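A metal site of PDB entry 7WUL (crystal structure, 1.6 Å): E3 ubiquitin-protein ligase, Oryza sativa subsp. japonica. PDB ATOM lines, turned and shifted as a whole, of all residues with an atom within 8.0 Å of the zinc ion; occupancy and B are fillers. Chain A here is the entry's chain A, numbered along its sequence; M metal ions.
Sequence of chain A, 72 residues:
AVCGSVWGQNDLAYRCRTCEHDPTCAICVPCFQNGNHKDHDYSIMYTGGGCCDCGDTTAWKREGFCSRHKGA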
ATOM      1  N   ARG A  15     -16.818  -3.288 -10.387  1.00  0.00           N
ATOM      2  CA  ARG A  15     -17.734  -4.041 -11.212  1.00  0.00           C
ATOM      3  C   ARG A  15     -16.986  -5.239 -11.768  1.00  0.00           C
ATOM      4  O   ARG A  15     -15.797  -5.147 -12.090  1.00  0.00           O
ATOM      5  CB  ARG A  15     -18.232  -3.214 -12.404  1.00  0.00           C
ATOM      6  CG  ARG A  15     -18.829  -1.877 -12.106  1.00  0.00           C
ATOM      7  CD  ARG A  15     -20.188  -1.954 -11.511  1.00  0.00           C
ATOM      8  NE  ARG A  15     -20.835  -0.647 -11.580  1.00  0.00           N
ATOM      9  CZ  ARG A  15     -21.957  -0.356 -10.936  1.00  0.00           C
ATOM     10  NH1 ARG A  15     -22.582  -1.265 -10.203  1.00  0.00           N
ATOM     11  NH2 ARG A  15     -22.431   0.885 -10.984  1.00  0.00           N
ATOM     12  N   CYS A  16     -17.686  -6.338 -11.934  1.00  0.00           N
ATOM     13  CA  CYS A  16     -17.140  -7.434 -12.731  1.00  0.00           C
ATOM     14  C   CYS A  16     -18.263  -7.977 -13.609  1.00  0.00           C
ATOM     15  O   CYS A  16     -19.188  -8.609 -13.086  1.00  0.00           O
ATOM     16  CB  CYS A  16     -16.549  -8.531 -11.862  1.00  0.00           C
ATOM     17  SG  CYS A  16     -15.668  -9.760 -12.856  1.00  0.00           S
ATOM     18  N   ARG A  17     -18.143  -7.730 -14.895  1.00  0.00           N
ATOM     19  CA  ARG A  17     -19.182  -8.245 -15.822  1.00  0.00           C
ATOM     20  C   ARG A  17     -19.185  -9.797 -15.966  1.00  0.00           C
ATOM     21  O   ARG A  17     -20.175 -10.482 -16.385  1.00  0.00           O
ATOM     22  CB  ARG A  17     -19.067  -7.585 -17.202  1.00  0.00           C
ATOM     23  CG  ARG A  17     -18.880  -6.060 -17.194  1.00  0.00           C
ATOM     24  CD  ARG A  17     -19.738  -5.409 -16.133  1.00  0.00           C
ATOM     25  NE  ARG A  17     -19.801  -3.951 -16.213  1.00  0.00           N
ATOM     26  CZ  ARG A  17     -20.741  -3.210 -15.625  1.00  0.00           C
ATOM     27  NH1 ARG A  17     -21.686  -3.754 -14.868  1.00  0.00           N
ATOM     28  NH2 ARG A  17     -20.709  -1.884 -15.772  1.00  0.00           N
ATOM     29  N   THR A  18     -18.050 -10.389 -15.600  1.00  0.00           N
ATOM     30  CA  THR A  18     -17.980 -11.843 -15.590  1.00  0.00           C
ATOM     31  C   THR A  18     -18.798 -12.414 -14.435  1.00  0.00           C
ATOM     32  O   THR A  18     -19.512 -13.415 -14.603  1.00  0.00           O
ATOM     33  CB  THR A  18     -16.520 -12.291 -15.493  1.00  0.00           C
ATOM     34  OG1 THR A  18     -15.756 -11.682 -16.552  1.00  0.00           O
ATOM     35  CG2 THR A  18     -16.391 -13.817 -15.561  1.00  0.00           C
ATOM     36  N   CYS A  19     -18.736 -11.786 -13.266  1.00  0.00           N
ATOM     37  CA  CYS A  19     -19.333 -12.344 -12.058  1.00  0.00           C
ATOM     38  C   CYS A  19     -20.725 -11.830 -11.759  1.00  0.00           C
ATOM     39  O   CYS A  19     -21.459 -12.488 -11.009  1.00  0.00           O
ATOM     40  CB  CYS A  19     -18.445 -12.039 -10.841  1.00  0.00           C
ATOM     41  SG  CYS A  19     -16.883 -12.947 -10.819  1.00  0.00           S
ATOM     42  N   GLU A  20     -21.116 -10.680 -12.316  1.00  0.00           N
ATOM     43  CA  GLU A  20     -22.341 -10.031 -11.889  1.00  0.00           C
ATOM     44  C   GLU A  20     -23.568 -10.776 -12.412  1.00  0.00           C
ATOM     45  O   GLU A  20     -23.531 -11.421 -13.467  1.00  0.00           O
ATOM     46  CB  GLU A  20     -22.395  -8.578 -12.381  1.00  0.00           C
ATOM     47  CG  GLU A  20     -22.785  -8.497 -13.858  1.00  0.00           C
ATOM     48  CD  GLU A  20     -22.553  -7.138 -14.512  1.00  0.00           C
ATOM     49  OE1 GLU A  20     -21.877  -6.258 -13.934  1.00  0.00           O
ATOM     50  OE2 GLU A  20     -23.110  -6.941 -15.621  1.00  0.00           O
ATOM     51  N   ILE A  27     -18.802  -5.113  -5.948  1.00  0.00           N
ATOM     52  CA  ILE A  27     -18.202  -5.576  -4.697  1.00  0.00           C
ATOM     53  C   ILE A  27     -17.135  -4.591  -4.243  1.00  0.00           C
ATOM     54  O   ILE A  27     -16.595  -3.809  -5.032  1.00  0.00           O
ATOM     55  CB  ILE A  27     -17.615  -7.009  -4.803  1.00  0.00           C
ATOM     56  CG1 ILE A  27     -16.432  -7.079  -5.788  1.00  0.00           C
ATOM     57  CG2 ILE A  27     -18.743  -8.019  -5.130  1.00  0.00           C
ATOM     58  CD1 ILE A  27     -15.754  -8.464  -5.814  1.00  0.00           C
ATOM     59  N   PHE A  32     -12.849  -7.681  -3.757  1.00  0.00           N
ATOM     60  CA  PHE A  32     -12.250  -7.970  -5.061  1.00  0.00           C
ATOM     61  C   PHE A  32     -10.819  -8.495  -4.907  1.00  0.00           C
ATOM     62  O   PHE A  32     -10.435  -9.500  -5.534  1.00  0.00           O
ATOM     63  CB  PHE A  32     -12.266  -6.717  -5.962  1.00  0.00           C
ATOM     64  CG  PHE A  32     -11.683  -6.980  -7.308  1.00  0.00           C
ATOM     65  CD1 PHE A  32     -10.322  -6.823  -7.561  1.00  0.00           C
ATOM     66  CD2 PHE A  32     -12.496  -7.482  -8.315  1.00  0.00           C
ATOM     67  CE1 PHE A  32      -9.789  -7.129  -8.820  1.00  0.00           C
ATOM     68  CE2 PHE A  32     -11.963  -7.776  -9.552  1.00  0.00           C
ATOM     69  CZ  PHE A  32     -10.616  -7.603  -9.796  1.00  0.00           C
ATOM     70  N   GLY A  35     -10.478 -12.070  -3.870  1.00  0.00           N
ATOM     71  CA  GLY A  35     -11.082 -13.018  -4.771  1.00  0.00           C
ATOM     72  C   GLY A  35     -10.247 -13.236  -6.031  1.00  0.00           C
ATOM     73  O   GLY A  35      -9.165 -12.685  -6.217  1.00  0.00           O
ATOM     74  N   ASN A  36     -10.803 -14.057  -6.916  1.00  0.00           N
ATOM     75  CA  ASN A  36     -10.095 -14.581  -8.079  1.00  0.00           C
ATOM     76  C   ASN A  36     -10.835 -14.113  -9.330  1.00  0.00           C
ATOM     77  O   ASN A  36     -11.885 -14.669  -9.665  1.00  0.00           O
ATOM     78  CB  ASN A  36     -10.025 -16.095  -8.025  1.00  0.00           C
ATOM     79  CG  ASN A  36      -9.402 -16.589  -6.742  1.00  0.00           C
ATOM     80  OD1 ASN A  36      -8.366 -16.076  -6.312  1.00  0.00           O
ATOM     81  ND2 ASN A  36     -10.028 -17.585  -6.102  1.00  0.00           N
ATOM     82  N   HIS A  37     -10.309 -13.088  -9.989  1.00  0.00           N
ATOM     83  CA  HIS A  37     -10.942 -12.526 -11.183  1.00  0.00           C
ATOM     84  C   HIS A  37      -9.943 -12.374 -12.317  1.00  0.00           C
ATOM     85  O   HIS A  37     -10.068 -11.463 -13.142  1.00  0.00           O
ATOM     86  CB  HIS A  37     -11.584 -11.172 -10.893  1.00  0.00           C
ATOM     87  CG  HIS A  37     -12.585 -11.195  -9.785  1.00  0.00           C
ATOM     88  ND1 HIS A  37     -13.938 -11.406  -9.992  1.00  0.00           N
ATOM     89  CD2 HIS A  37     -12.416 -11.077  -8.448  1.00  0.00           C
ATOM     90  CE1 HIS A  37     -14.556 -11.420  -8.823  1.00  0.00           C
ATOM     91  NE2 HIS A  37     -13.661 -11.223  -7.877  1.00  0.00           N
ATOM     92  N   LYS A  38      -8.949 -13.246 -12.371  1.00  0.00           N
ATOM     93  CA  LYS A  38      -7.983 -13.125 -13.455  1.00  0.00           C
ATOM     94  C   LYS A  38      -8.647 -13.514 -14.776  1.00  0.00           C
ATOM     95  O   LYS A  38      -9.395 -14.500 -14.867  1.00  0.00           O
ATOM     96  CB  LYS A  38      -6.721 -13.923 -13.179  1.00  0.00           C
ATOM     97  CG  LYS A  38      -5.915 -13.361 -12.000  1.00  0.00           C
ATOM     98  CD  LYS A  38      -4.625 -14.118 -11.743  1.00  0.00           C
ATOM     99  CE  LYS A  38      -3.888 -13.530 -10.556  1.00  0.00           C
ATOM    100  NZ  LYS A  38      -2.834 -14.455 -10.024  1.00  0.00           N
ATOM    101  N   ASP A  39      -8.434 -12.663 -15.767  1.00  0.00           N
ATOM    102  CA  ASP A  39      -9.049 -12.735 -17.078  1.00  0.00           C
ATOM    103  C   ASP A  39     -10.522 -12.364 -17.054  1.00  0.00           C
ATOM    104  O   ASP A  39     -11.206 -12.497 -18.057  1.00  0.00           O
ATOM    105  CB  ASP A  39      -8.861 -14.129 -17.685  1.00  0.00           C
ATOM    106  CG  ASP A  39      -7.571 -14.245 -18.485  1.00  0.00           C
ATOM    107  OD1 ASP A  39      -7.027 -13.190 -18.909  1.00  0.00           O
ATOM    108  OD2 ASP A  39      -7.093 -15.382 -18.703  1.00  0.00           O
ATOM    109  N   HIS A  40     -11.035 -11.881 -15.913  1.00  0.00           N
ATOM    110  CA  HIS A  40     -12.411 -11.400 -15.914  1.00  0.00           C
ATOM    111  C   HIS A  40     -12.514  -9.993 -16.506  1.00  0.00           C
ATOM    112  O   HIS A  40     -11.547  -9.227 -16.537  1.00  0.00           O
ATOM    113  CB  HIS A  40     -12.987 -11.356 -14.491  1.00  0.00           C
ATOM    114  CG  HIS A  40     -13.203 -12.695 -13.892  1.00  0.00           C
ATOM    115  ND1 HIS A  40     -14.029 -12.880 -12.804  1.00  0.00           N
ATOM    116  CD2 HIS A  40     -12.735 -13.913 -14.226  1.00  0.00           C
ATOM    117  CE1 HIS A  40     -14.044 -14.167 -12.483  1.00  0.00           C
ATOM    118  NE2 HIS A  40     -13.284 -14.817 -13.350  1.00  0.00           N
ATOM    119  N   ASP A  41     -13.731  -9.659 -16.944  1.00  0.00           N
ATOM    120  CA  ASP A  41     -14.032  -8.305 -17.423  1.00  0.00           C
ATOM    121  C   ASP A  41     -14.431  -7.438 -16.228  1.00  0.00           C
ATOM    122  O   ASP A  41     -15.605  -7.154 -15.990  1.00  0.00           O
ATOM    123  CB  ASP A  41     -15.130  -8.337 -18.459  1.00  0.00           C
ATOM    124  CG  ASP A  41     -15.502  -6.958 -18.962  1.00  0.00           C
ATOM    125  OD1 ASP A  41     -14.679  -6.031 -18.830  1.00  0.00           O
ATOM    126  OD2 ASP A  41     -16.615  -6.809 -19.502  1.00  0.00           O
ATOM    127  N   TYR A  42     -13.431  -7.001 -15.485  1.00  0.00           N
ATOM    128  CA  TYR A  42     -13.688  -6.197 -14.296  1.00  0.00           C
ATOM    129  C   TYR A  42     -13.166  -4.782 -14.493  1.00  0.00           C
ATOM    130  O   TYR A  42     -12.289  -4.521 -15.312  1.00  0.00           O
ATOM    131  CB  TYR A  42     -13.036  -6.806 -13.062  1.00  0.00           C
ATOM    132  CG  TYR A  42     -11.520  -6.851 -13.077  1.00  0.00           C
ATOM    133  CD1 TYR A  42     -10.772  -5.729 -12.721  1.00  0.00           C
ATOM    134  CD2 TYR A  42     -10.852  -8.012 -13.419  1.00  0.00           C
ATOM    135  CE1 TYR A  42      -9.383  -5.773 -12.724  1.00  0.00           C
ATOM    136  CE2 TYR A  42      -9.480  -8.067 -13.427  1.00  0.00           C
ATOM    137  CZ  TYR A  42      -8.745  -6.953 -13.085  1.00  0.00           C
ATOM    138  OH  TYR A  42      -7.371  -7.043 -13.108  1.00  0.00           O
ATOM    139  N   TRP A  60     -24.300 -12.303  -7.386  1.00  0.00           N
ATOM    140  CA  TRP A  60     -22.904 -12.459  -7.773  1.00  0.00           C
ATOM    141  C   TRP A  60     -22.603 -13.946  -7.879  1.00  0.00           C
ATOM    142  O   TRP A  60     -23.047 -14.736  -7.027  1.00  0.00           O
ATOM    143  CB  TRP A  60     -22.014 -11.800  -6.708  1.00  0.00           C
ATOM    144  CG  TRP A  60     -20.622 -11.411  -7.110  1.00  0.00           C
ATOM    145  CD1 TRP A  60     -19.474 -12.104  -6.848  1.00  0.00           C
ATOM    146  CD2 TRP A  60     -20.218 -10.202  -7.764  1.00  0.00           C
ATOM    147  NE1 TRP A  60     -18.387 -11.415  -7.336  1.00  0.00           N
ATOM    148  CE2 TRP A  60     -18.818 -10.242  -7.889  1.00  0.00           C
ATOM    149  CE3 TRP A  60     -20.897  -9.093  -8.259  1.00  0.00           C
ATOM    150  CZ2 TRP A  60     -18.095  -9.207  -8.490  1.00  0.00           C
ATOM    151  CZ3 TRP A  60     -20.179  -8.073  -8.853  1.00  0.00           C
ATOM    152  CH2 TRP A  60     -18.797  -8.136  -8.953  1.00  0.00           C
ATOM    153  N   LYS A  61     -21.836 -14.333  -8.887  1.00  0.00           N
ATOM    154  CA  LYS A  61     -21.495 -15.737  -9.057  1.00  0.00           C
ATOM    155  C   LYS A  61     -20.605 -16.229  -7.918  1.00  0.00           C
ATOM    156  O   LYS A  61     -19.741 -15.505  -7.419  1.00  0.00           O
ATOM    157  CB  LYS A  61     -20.813 -15.961 -10.405  1.00  0.00           C
ATOM    158  CG  LYS A  61     -21.787 -15.915 -11.567  1.00  0.00           C
ATOM    159  CD  LYS A  61     -21.046 -15.922 -12.885  1.00  0.00           C
ATOM    160  CE  LYS A  61     -21.886 -15.253 -13.959  1.00  0.00           C
ATOM    161  NZ  LYS A  61     -21.313 -15.452 -15.329  1.00  0.00           N
ATOM    162  N   GLU A  63     -18.203 -18.333  -7.892  1.00  0.00           N
ATOM    163  CA  GLU A  63     -16.780 -18.363  -8.227  1.00  0.00           C
ATOM    164  C   GLU A  63     -16.116 -17.024  -7.976  1.00  0.00           C
ATOM    165  O   GLU A  63     -14.892 -16.968  -7.819  1.00  0.00           O
ATOM    166  CB  GLU A  63     -16.593 -18.802  -9.676  1.00  0.00           C
ATOM    167  CG  GLU A  63     -17.476 -18.039 -10.655  1.00  0.00           C
ATOM    168  CD  GLU A  63     -16.855 -16.721 -11.121  1.00  0.00           C
ATOM    169  OE1 GLU A  63     -17.588 -15.899 -11.716  1.00  0.00           O
ATOM    170  OE2 GLU A  63     -15.640 -16.526 -10.875  1.00  0.00           O
ATOM    171  N   GLY A  64     -16.895 -15.943  -7.939  1.00  0.00           N
ATOM    172  CA  GLY A  64     -16.369 -14.621  -7.723  1.00  0.00           C
ATOM    173  C   GLY A  64     -16.418 -14.141  -6.288  1.00  0.00           C
ATOM    174  O   GLY A  64     -16.129 -12.961  -6.042  1.00  0.00           O
ATOM    175  N   PHE A  65     -16.793 -14.991  -5.334  1.00  0.00           N
ATOM    176  CA  PHE A  65     -16.759 -14.625  -3.925  1.00  0.00           C
ATOM    177  C   PHE A  65     -15.318 -14.575  -3.428  1.00  0.00           C
ATOM    178  O   PHE A  65     -14.475 -15.398  -3.811  1.00  0.00           O
ATOM    179  CB  PHE A  65     -17.531 -15.637  -3.063  1.00  0.00           C
ATOM    180  CG  PHE A  65     -19.015 -15.697  -3.323  1.00  0.00           C
ATOM    181  CD1 PHE A  65     -19.658 -14.750  -4.109  1.00  0.00           C
ATOM    182  CD2 PHE A  65     -19.776 -16.697  -2.716  1.00  0.00           C
ATOM    183  CE1 PHE A  65     -21.031 -14.832  -4.325  1.00  0.00           C
ATOM    184  CE2 PHE A  65     -21.149 -16.766  -2.920  1.00  0.00           C
ATOM    185  CZ  PHE A  65     -21.776 -15.834  -3.724  1.00  0.00           C
HETATM  186 ZN    ZN M   1     -15.146 -11.607 -11.622  1.00  0.00          ZN
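Along chain A the residues within 4 Å of the zinc ion span positions 16 to 40.
The zinc ion is bound by ND1 of His 37 (2.0 Å), ND1 of His 40 (2.1 Å), SG of Cys 16 (2.3 Å) and SG of Cys 19 (2.3 Å). The zinc ion has four donor atoms within binding distance.
The side-chain sulfur of Cys 16 sits close to the backbone NH of Thr 18 (3.7 Å). SG of Cys 19 lies close to OE1 of Glu 63 (3.2 Å). N of Lys 61 lies within hydrogen-bond range of O of Cys 19.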
